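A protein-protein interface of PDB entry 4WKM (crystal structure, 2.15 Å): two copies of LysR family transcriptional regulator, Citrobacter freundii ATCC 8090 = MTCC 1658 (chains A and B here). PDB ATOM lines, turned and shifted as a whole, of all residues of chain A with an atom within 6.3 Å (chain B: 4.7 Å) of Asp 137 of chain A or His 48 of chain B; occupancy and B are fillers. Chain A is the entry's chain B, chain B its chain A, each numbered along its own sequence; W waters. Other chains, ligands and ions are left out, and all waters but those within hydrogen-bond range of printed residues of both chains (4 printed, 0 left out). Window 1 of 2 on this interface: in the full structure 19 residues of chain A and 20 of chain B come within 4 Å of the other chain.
OH of Tyr 110 of chain A touches CB of Ser 46 of chain B (3.5 Å). Val 135 of chain A touches Ser 46 of chain B. Thr 47 of chain B touches Phe 136 of chain A. OD2 of Asp 137 of chain A touches C of His 48 of chain B, at 3.6 Å. OD2 of Asp 137 of chain A touches N of Asn 49 of chain B (3.5 Å).
Asn 49 of chain A touches its own counterpart, Asn 49 of chain B. 4 positions are printed for both chains.
Hydrophobic or aromatic side chains of chain A within 4 Å of the printed part of chain B: Tyr 110 and Phe 136. Along chain B the printed residues that touch a printed residue of chain A span positions 46 to 49.
OH of Tyr 110 of chain A is in hydrogen-bond range of O of Thr 47 of chain B, 2.7 Å away. The backbone NH (N) of Thr 47 of chain B is in hydrogen-bond range of the backbone carbonyl oxygen (O) of Val 135 of chain A (2.9 Å). OG1 of Thr 47 of chain B is in hydrogen-bond range of OD1 of Asp 137 of chain A (2.7 Å). The side-chain amide nitrogen of Asn 49 of chain B sits close to the side-chain amide nitrogen of Asn 49 of chain A (3.1 Å).
Of the printed residues of chain B, Asn 49 of chain A touches Asn 49 (3.1 Å). Printed residues of chain B within 4 Å of Tyr 110 of chain A: Ser 46 (3.5 Å) and Thr 47 (2.7 Å). Of the printed residues of chain B, Phe 136 of chain A touches Thr 47. Printed residues of chain A within 4 Å of Thr 47 of chain B: Tyr 110, Val 135, Phe 136 and Asp 137. Printed residues of chain A within 4 Å of His 48 of chain B: Asp 137 (3.6 Å). Printed residues of chain A within 4 Å of Asn 49 of chain B: Asn 49 (3.1 Å) and Asp 137 (3.5 Å). The nearest printed residue of chain B that does not touch Asp 137 of chain A is Gly 20 of chain B (5.3 Å). The nearest printed residue of chain B that does not touch Tyr 110 of chain A is His 48 of chain B (4.6 Å).
N of Val 18 of chain B sits at hydrogen-bond distance from O of Ser 46 of chain B (2.7 Å). The backbone NH (N) of His 48 of chain B lies within hydrogen-bond range of the backbone carbonyl oxygen (O) of Val 18 of chain B (3.1 Å). A ring nitrogen (ND1) of His 48 of chain B lies within hydrogen-bond range of the backbone NH of Asn 50 of chain B (3.0 Å). The backbone NH (N) of Arg 51 of chain B sits close to the side-chain amide oxygen (OD1) of Asn 49 of chain B, 3.5 Å away. ND2 of Asn 49 of chain A sits at hydrogen-bond distance from OD2 of Asp 137 of chain A, 3.2 Å away. N of Phe 136 of chain A sits at hydrogen-bond distance from O of Arg 108 of chain A.
Water W2 lies within hydrogen-bond range of OG of Ser 46 of chain B and OH of Tyr 110 of chain A. Water W3 bridges the side-chain amide nitrogen (ND2) of Asn 49 of chain B and the side-chain amide oxygen (OD1) of Asn 49 of chain A. Water W1 bridges the side-chain amide oxygen of Asn 49 of chain A (2.9 Å) and the side-chain amide oxygen of Asn 49 of chain B (3.0 Å). Water W4 lies within hydrogen-bond range of ND2 of Asn 49 of chain A, OD1 of Asn 49 of chain B and O of Arg 51 of chain B.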
ATOM      1  N   VAL A  19     -13.246  -7.932  -3.907  1.00  0.00           N
ATOM      2  CA  VAL A  19     -13.968  -8.765  -2.964  1.00  0.00           C
ATOM      3  C   VAL A  19     -13.294  -8.591  -1.604  1.00  0.00           C
ATOM      4  O   VAL A  19     -12.075  -8.552  -1.507  1.00  0.00           O
ATOM      5  CB  VAL A  19     -14.054 -10.252  -3.381  1.00  0.00           C
ATOM      6  CG1 VAL A  19     -12.639 -10.916  -3.584  1.00  0.00           C
ATOM      7  CG2 VAL A  19     -14.898 -11.017  -2.345  1.00  0.00           C
ATOM      8  N   HIS A  48     -16.660  -5.347  -2.338  1.00  0.00           N
ATOM      9  CA  HIS A  48     -17.939  -5.990  -2.605  1.00  0.00           C
ATOM     10  C   HIS A  48     -17.932  -7.391  -1.996  1.00  0.00           C
ATOM     11  O   HIS A  48     -16.900  -7.840  -1.460  1.00  0.00           O
ATOM     12  CB  HIS A  48     -18.239  -6.034  -4.114  1.00  0.00           C
ATOM     13  CG  HIS A  48     -17.181  -6.707  -4.947  1.00  0.00           C
ATOM     14  ND1 HIS A  48     -17.122  -8.078  -5.116  1.00  0.00           N
ATOM     15  CD2 HIS A  48     -16.179  -6.194  -5.708  1.00  0.00           C
ATOM     16  CE1 HIS A  48     -16.108  -8.379  -5.910  1.00  0.00           C
ATOM     17  NE2 HIS A  48     -15.517  -7.258  -6.282  1.00  0.00           N
ATOM     18  N   ASN A  49     -19.075  -8.073  -2.103  1.00  0.00           N
ATOM     19  CA  ASN A  49     -19.268  -9.376  -1.513  1.00  0.00           C
ATOM     20  C   ASN A  49     -19.313 -10.477  -2.593  1.00  0.00           C
ATOM     21  O   ASN A  49     -19.992 -11.491  -2.429  1.00  0.00           O
ATOM     22  CB  ASN A  49     -20.558  -9.401  -0.639  1.00  0.00           C
ATOM     23  CG  ASN A  49     -21.829  -9.228  -1.420  1.00  0.00           C
ATOM     24  OD1 ASN A  49     -21.822  -9.083  -2.630  1.00  0.00           O
ATOM     25  ND2 ASN A  49     -22.964  -9.230  -0.702  1.00  0.00           N
ATOM     26  N   ASN A  50     -18.552 -10.249  -3.672  1.00  0.00           N
ATOM     27  CA  ASN A  50     -18.456 -11.106  -4.868  1.00  0.00           C
ATOM     28  C   ASN A  50     -19.686 -11.114  -5.756  1.00  0.00           C
ATOM     29  O   ASN A  50     -19.705 -11.822  -6.752  1.00  0.00           O
ATOM     30  CB  ASN A  50     -18.133 -12.564  -4.501  1.00  0.00           C
ATOM     31  CG  ASN A  50     -17.121 -13.181  -5.458  1.00  0.00           C
ATOM     32  OD1 ASN A  50     -16.078 -12.584  -5.743  1.00  0.00           O
ATOM     33  ND2 ASN A  50     -17.413 -14.384  -5.933  1.00  0.00           N
ATOM     34  N   ARG A 108     -21.124 -21.558   5.786  1.00  0.00           N
ATOM     35  CA  ARG A 108     -20.835 -21.630   4.380  1.00  0.00           C
ATOM     36  C   ARG A 108     -21.193 -20.338   3.675  1.00  0.00           C
ATOM     37  O   ARG A 108     -21.751 -19.417   4.269  1.00  0.00           O
ATOM     38  CB  ARG A 108     -21.618 -22.763   3.773  1.00  0.00           C
ATOM     39  CG  ARG A 108     -23.064 -22.636   4.091  1.00  0.00           C
ATOM     40  CD  ARG A 108     -23.858 -23.599   3.303  1.00  0.00           C
ATOM     41  NE  ARG A 108     -24.082 -23.074   1.996  1.00  0.00           N
ATOM     42  CZ  ARG A 108     -25.012 -23.533   1.191  1.00  0.00           C
ATOM     43  NH1 ARG A 108     -25.810 -24.528   1.582  1.00  0.00           N
ATOM     44  NH2 ARG A 108     -25.129 -22.987  -0.006  1.00  0.00           N
ATOM     45  N   SER A 109     -20.894 -20.286   2.391  1.00  0.00           N
ATOM     46  CA  SER A 109     -21.208 -19.150   1.583  1.00  0.00           C
ATOM     47  C   SER A 109     -22.445 -19.506   0.782  1.00  0.00           C
ATOM     48  O   SER A 109     -23.025 -20.568   0.983  1.00  0.00           O
ATOM     49  CB  SER A 109     -20.029 -18.795   0.703  1.00  0.00           C
ATOM     50  OG  SER A 109     -19.911 -19.699  -0.387  1.00  0.00           O
ATOM     51  N   TYR A 110     -22.865 -18.629  -0.114  1.00  0.00           N
ATOM     52  CA  TYR A 110     -24.027 -18.900  -0.940  1.00  0.00           C
ATOM     53  C   TYR A 110     -23.722 -19.926  -2.039  1.00  0.00           C
ATOM     54  O   TYR A 110     -24.648 -20.407  -2.706  1.00  0.00           O
ATOM     55  CB  TYR A 110     -24.531 -17.622  -1.600  1.00  0.00           C
ATOM     56  CG  TYR A 110     -25.273 -16.695  -0.679  1.00  0.00           C
ATOM     57  CD1 TYR A 110     -24.608 -15.951   0.273  1.00  0.00           C
ATOM     58  CD2 TYR A 110     -26.640 -16.555  -0.783  1.00  0.00           C
ATOM     59  CE1 TYR A 110     -25.286 -15.114   1.116  1.00  0.00           C
ATOM     60  CE2 TYR A 110     -27.330 -15.728   0.047  1.00  0.00           C
ATOM     61  CZ  TYR A 110     -26.655 -15.008   1.000  1.00  0.00           C
ATOM     62  OH  TYR A 110     -27.384 -14.165   1.813  1.00  0.00           O
ATOM     63  N   VAL A 135     -25.509 -19.265   6.336  1.00  0.00           N
ATOM     64  CA  VAL A 135     -24.991 -18.828   5.043  1.00  0.00           C
ATOM     65  C   VAL A 135     -24.478 -17.385   5.112  1.00  0.00           C
ATOM     66  O   VAL A 135     -25.151 -16.518   5.660  1.00  0.00           O
ATOM     67  CB  VAL A 135     -26.072 -18.946   3.969  1.00  0.00           C
ATOM     68  CG1 VAL A 135     -25.527 -18.501   2.574  1.00  0.00           C
ATOM     69  CG2 VAL A 135     -26.602 -20.389   3.896  1.00  0.00           C
ATOM     70  N   PHE A 136     -23.295 -17.143   4.540  1.00  0.00           N
ATOM     71  CA  PHE A 136     -22.618 -15.849   4.587  1.00  0.00           C
ATOM     72  C   PHE A 136     -22.284 -15.319   3.212  1.00  0.00           C
ATOM     73  O   PHE A 136     -21.896 -16.082   2.323  1.00  0.00           O
ATOM     74  CB  PHE A 136     -21.331 -15.957   5.399  1.00  0.00           C
ATOM     75  CG  PHE A 136     -21.556 -16.202   6.853  1.00  0.00           C
ATOM     76  CD1 PHE A 136     -21.729 -17.481   7.308  1.00  0.00           C
ATOM     77  CD2 PHE A 136     -21.636 -15.140   7.762  1.00  0.00           C
ATOM     78  CE1 PHE A 136     -21.948 -17.746   8.627  1.00  0.00           C
ATOM     79  CE2 PHE A 136     -21.857 -15.386   9.103  1.00  0.00           C
ATOM     80  CZ  PHE A 136     -22.016 -16.693   9.545  1.00  0.00           C
ATOM     81  N   ASP A 137     -22.396 -14.001   3.062  1.00  0.00           N
ATOM     82  CA  ASP A 137     -22.159 -13.295   1.795  1.00  0.00           C
ATOM     83  C   ASP A 137     -20.701 -12.908   1.669  1.00  0.00           C
ATOM     84  O   ASP A 137     -20.237 -12.469   0.621  1.00  0.00           O
ATOM     85  CB  ASP A 137     -23.038 -12.037   1.688  1.00  0.00           C
ATOM     86  CG  ASP A 137     -22.679 -10.956   2.723  1.00  0.00           C
ATOM     87  OD1 ASP A 137     -22.715 -11.216   3.940  1.00  0.00           O
ATOM     88  OD2 ASP A 137     -22.319  -9.838   2.326  1.00  0.00           O
ATOM     89  N   SER A 138     -19.979 -13.056   2.761  1.00  0.00           N
ATOM     90  CA  SER A 138     -18.609 -12.649   2.818  1.00  0.00           C
ATOM     91  C   SER A 138     -17.869 -13.539   3.765  1.00  0.00           C
ATOM     92  O   SER A 138     -18.345 -13.807   4.883  1.00  0.00           O
ATOM     93  CB  SER A 138     -18.519 -11.186   3.267  1.00  0.00           C
ATOM     94  OG  SER A 138     -17.249 -10.856   3.778  1.00  0.00           O
ATOM     95  N   SER A 139     -16.705 -14.016   3.335  1.00  0.00           N
ATOM     96  CA  SER A 139     -15.889 -14.833   4.217  1.00  0.00           C
ATOM     97  C   SER A 139     -15.399 -14.027   5.410  1.00  0.00           C
ATOM     98  O   SER A 139     -15.144 -14.603   6.475  1.00  0.00           O
ATOM     99  CB  SER A 139     -14.691 -15.452   3.459  1.00  0.00           C
ATOM    100  OG  SER A 139     -15.156 -16.391   2.501  1.00  0.00           O
ATOM    101  N   THR A 141     -17.076 -11.845   7.286  1.00  0.00           N
ATOM    102  CA  THR A 141     -18.161 -11.961   8.264  1.00  0.00           C
ATOM    103  C   THR A 141     -18.180 -13.404   8.796  1.00  0.00           C
ATOM    104  O   THR A 141     -18.199 -13.606  10.009  1.00  0.00           O
ATOM    105  CB  THR A 141     -19.550 -11.596   7.642  1.00  0.00           C
ATOM    106  OG1 THR A 141     -19.495 -10.305   7.026  1.00  0.00           O
ATOM    107  CG2 THR A 141     -20.674 -11.587   8.677  1.00  0.00           C
ATOM    108  N   GLY B  17     -32.738 -13.051   6.535  1.00  0.00           N
ATOM    109  CA  GLY B  17     -31.514 -12.459   6.029  1.00  0.00           C
ATOM    110  C   GLY B  17     -31.102 -11.247   6.846  1.00  0.00           C
ATOM    111  O   GLY B  17     -31.876 -10.324   6.999  1.00  0.00           O
ATOM    112  N   VAL B  18     -29.865 -11.242   7.323  1.00  0.00           N
ATOM    113  CA  VAL B  18     -29.354 -10.253   8.263  1.00  0.00           C
ATOM    114  C   VAL B  18     -28.140  -9.522   7.742  1.00  0.00           C
ATOM    115  O   VAL B  18     -27.133 -10.158   7.391  1.00  0.00           O
ATOM    116  CB  VAL B  18     -28.946 -10.940   9.598  1.00  0.00           C
ATOM    117  CG1 VAL B  18     -28.717  -9.911  10.678  1.00  0.00           C
ATOM    118  CG2 VAL B  18     -29.994 -11.927  10.030  1.00  0.00           C
ATOM    119  N   VAL B  19     -28.183  -8.189   7.771  1.00  0.00           N
ATOM    120  CA  VAL B  19     -27.023  -7.408   7.402  1.00  0.00           C
ATOM    121  C   VAL B  19     -25.882  -7.812   8.338  1.00  0.00           C
ATOM    122  O   VAL B  19     -26.103  -8.013   9.532  1.00  0.00           O
ATOM    123  CB  VAL B  19     -27.311  -5.880   7.436  1.00  0.00           C
ATOM    124  CG1 VAL B  19     -27.804  -5.378   8.831  1.00  0.00           C
ATOM    125  CG2 VAL B  19     -26.102  -5.108   6.926  1.00  0.00           C
ATOM    126  N   GLY B  20     -24.674  -7.981   7.791  1.00  0.00           N
ATOM    127  CA  GLY B  20     -23.621  -8.664   8.496  1.00  0.00           C
ATOM    128  C   GLY B  20     -23.213  -8.020   9.793  1.00  0.00           C
ATOM    129  O   GLY B  20     -22.868  -8.714  10.765  1.00  0.00           O
ATOM    130  N   SER B  46     -29.169 -16.206   6.901  1.00  0.00           N
ATOM    131  CA  SER B  46     -28.199 -15.773   5.900  1.00  0.00           C
ATOM    132  C   SER B  46     -27.792 -14.350   6.153  1.00  0.00           C
ATOM    133  O   SER B  46     -28.555 -13.587   6.761  1.00  0.00           O
ATOM    134  CB  SER B  46     -28.735 -15.911   4.476  1.00  0.00           C
ATOM    135  OG  SER B  46     -29.994 -15.319   4.287  1.00  0.00           O
ATOM    136  N   THR B  47     -26.591 -13.976   5.731  1.00  0.00           N
ATOM    137  CA  THR B  47     -26.213 -12.562   5.825  1.00  0.00           C
ATOM    138  C   THR B  47     -26.128 -11.896   4.461  1.00  0.00           C
ATOM    139  O   THR B  47     -25.948 -12.558   3.420  1.00  0.00           O
ATOM    140  CB  THR B  47     -24.851 -12.337   6.548  1.00  0.00           C
ATOM    141  OG1 THR B  47     -23.781 -12.889   5.762  1.00  0.00           O
ATOM    142  CG2 THR B  47     -24.866 -12.931   7.998  1.00  0.00           C
ATOM    143  N   HIS B  48     -26.239 -10.572   4.482  1.00  0.00           N
ATOM    144  CA  HIS B  48     -26.171  -9.772   3.280  1.00  0.00           C
ATOM    145  C   HIS B  48     -25.424  -8.492   3.596  1.00  0.00           C
ATOM    146  O   HIS B  48     -25.084  -8.255   4.752  1.00  0.00           O
ATOM    147  CB  HIS B  48     -27.562  -9.513   2.738  1.00  0.00           C
ATOM    148  CG  HIS B  48     -28.492  -8.870   3.712  1.00  0.00           C
ATOM    149  ND1 HIS B  48     -28.408  -7.535   4.053  1.00  0.00           N
ATOM    150  CD2 HIS B  48     -29.545  -9.367   4.401  1.00  0.00           C
ATOM    151  CE1 HIS B  48     -29.373  -7.240   4.904  1.00  0.00           C
ATOM    152  NE2 HIS B  48     -30.084  -8.334   5.126  1.00  0.00           N
ATOM    153  N   ASN B  49     -25.121  -7.689   2.579  1.00  0.00           N
ATOM    154  CA  ASN B  49     -24.371  -6.457   2.814  1.00  0.00           C
ATOM    155  C   ASN B  49     -25.259  -5.210   2.684  1.00  0.00           C
ATOM    156  O   ASN B  49     -24.793  -4.133   2.328  1.00  0.00           O
ATOM    157  CB  ASN B  49     -23.162  -6.377   1.873  1.00  0.00           C
ATOM    158  CG  ASN B  49     -23.539  -6.306   0.387  1.00  0.00           C
ATOM    159  OD1 ASN B  49     -24.712  -6.378   0.009  1.00  0.00           O
ATOM    160  ND2 ASN B  49     -22.525  -6.154  -0.463  1.00  0.00           N
ATOM    161  N   ASN B  50     -26.534  -5.406   2.989  1.00  0.00           N
ATOM    162  CA  ASN B  50     -27.591  -4.379   3.062  1.00  0.00           C
ATOM    163  C   ASN B  50     -28.222  -4.068   1.712  1.00  0.00           C
ATOM    164  O   ASN B  50     -29.164  -3.291   1.649  1.00  0.00           O
ATOM    165  CB  ASN B  50     -27.111  -3.089   3.683  1.00  0.00           C
ATOM    166  CG  ASN B  50     -28.210  -2.402   4.499  1.00  0.00           C
ATOM    167  OD1 ASN B  50     -28.994  -3.057   5.168  1.00  0.00           O
ATOM    168  ND2 ASN B  50     -28.257  -1.085   4.437  1.00  0.00           N
ATOM    169  N   ARG B  51     -27.687  -4.670   0.646  1.00  0.00           N
ATOM    170  CA  ARG B  51     -28.399  -4.763  -0.641  1.00  0.00           C
ATOM    171  C   ARG B  51     -28.913  -6.196  -0.777  1.00  0.00           C
ATOM    172  O   ARG B  51     -28.135  -7.115  -0.842  1.00  0.00           O
ATOM    173  CB  ARG B  51     -27.495  -4.415  -1.820  1.00  0.00           C
ATOM    174  CG  ARG B  51     -28.120  -4.800  -3.159  1.00  0.00           C
ATOM    175  CD  ARG B  51     -27.355  -4.220  -4.320  1.00  0.00           C
ATOM    176  NE  ARG B  51     -28.076  -4.419  -5.575  1.00  0.00           N
ATOM    177  CZ  ARG B  51     -28.104  -3.546  -6.582  1.00  0.00           C
ATOM    178  NH1 ARG B  51     -27.443  -2.396  -6.490  1.00  0.00           N
ATOM    179  NH2 ARG B  51     -28.804  -3.824  -7.682  1.00  0.00           N
ATOM    180  N   VAL B  52     -30.223  -6.376  -0.760  1.00  0.00           N
ATOM    181  CA  VAL B  52     -30.817  -7.685  -0.628  1.00  0.00           C
ATOM    182  C   VAL B  52     -32.177  -7.704  -1.321  1.00  0.00           C
ATOM    183  O   VAL B  52     -32.886  -6.687  -1.334  1.00  0.00           O
ATOM    184  CB  VAL B  52     -30.974  -8.067   0.865  1.00  0.00           C
ATOM    185  CG1 VAL B  52     -31.677  -6.938   1.659  1.00  0.00           C
ATOM    186  CG2 VAL B  52     -31.675  -9.421   1.027  1.00  0.00           C
ATOM    187  N   THR B  62     -36.245  -9.648   6.756  1.00  0.00           N
ATOM    188  CA  THR B  62     -34.935  -9.075   6.493  1.00  0.00           C
ATOM    189  C   THR B  62     -34.513  -8.110   7.606  1.00  0.00           C
ATOM    190  O   THR B  62     -35.228  -7.148   7.874  1.00  0.00           O
ATOM    191  CB  THR B  62     -34.946  -8.310   5.165  1.00  0.00           C
ATOM    192  OG1 THR B  62     -35.407  -9.170   4.126  1.00  0.00           O
ATOM    193  CG2 THR B  62     -33.580  -7.771   4.827  1.00  0.00           C
ATOM    194  N   ILE B  63     -33.375  -8.336   8.250  1.00  0.00           N
ATOM    195  CA  ILE B  63     -32.823  -7.342   9.161  1.00  0.00           C
ATOM    196  C   ILE B  63     -31.846  -6.464   8.379  1.00  0.00           C
ATOM    197  O   ILE B  63     -30.921  -6.953   7.716  1.00  0.00           O
ATOM    198  CB  ILE B  63     -32.168  -7.975  10.367  1.00  0.00           C
ATOM    199  CG1 ILE B  63     -33.223  -8.695  11.180  1.00  0.00           C
ATOM    200  CG2 ILE B  63     -31.524  -6.917  11.242  1.00  0.00           C
ATOM    201  CD1 ILE B  63     -32.676  -9.424  12.375  1.00  0.00           C
ATOM    202  N   ARG B  64     -32.089  -5.157   8.409  1.00  0.00           N
ATOM    203  CA  ARG B  64     -31.347  -4.254   7.582  1.00  0.00           C
ATOM    204  C   ARG B  64     -31.193  -2.871   8.161  1.00  0.00           C
ATOM    205  O   ARG B  64     -31.831  -2.533   9.165  1.00  0.00           O
ATOM    206  CB  ARG B  64     -32.014  -4.189   6.220  1.00  0.00           C
ATOM    207  CG  ARG B  64     -33.217  -3.331   6.140  1.00  0.00           C
ATOM    208  CD  ARG B  64     -34.222  -3.922   5.184  1.00  0.00           C
ATOM    209  NE  ARG B  64     -33.780  -3.822   3.801  1.00  0.00           N
ATOM    210  CZ  ARG B  64     -34.545  -4.120   2.752  1.00  0.00           C
ATOM    211  NH1 ARG B  64     -34.063  -3.980   1.525  1.00  0.00           N
ATOM    212  NH2 ARG B  64     -35.783  -4.559   2.921  1.00  0.00           N
HETATM  213  O   HOH W   1     -24.245  -7.410  -2.791  1.00  0.00           O
HETATM  214  O   HOH W   2     -29.757 -12.652   3.180  1.00  0.00           O
HETATM  215  O   HOH W   3     -21.436  -5.855  -3.181  1.00  0.00           O
HETATM  216  O   HOH W   4     -25.862  -9.204  -0.131  1.00  0.00           O
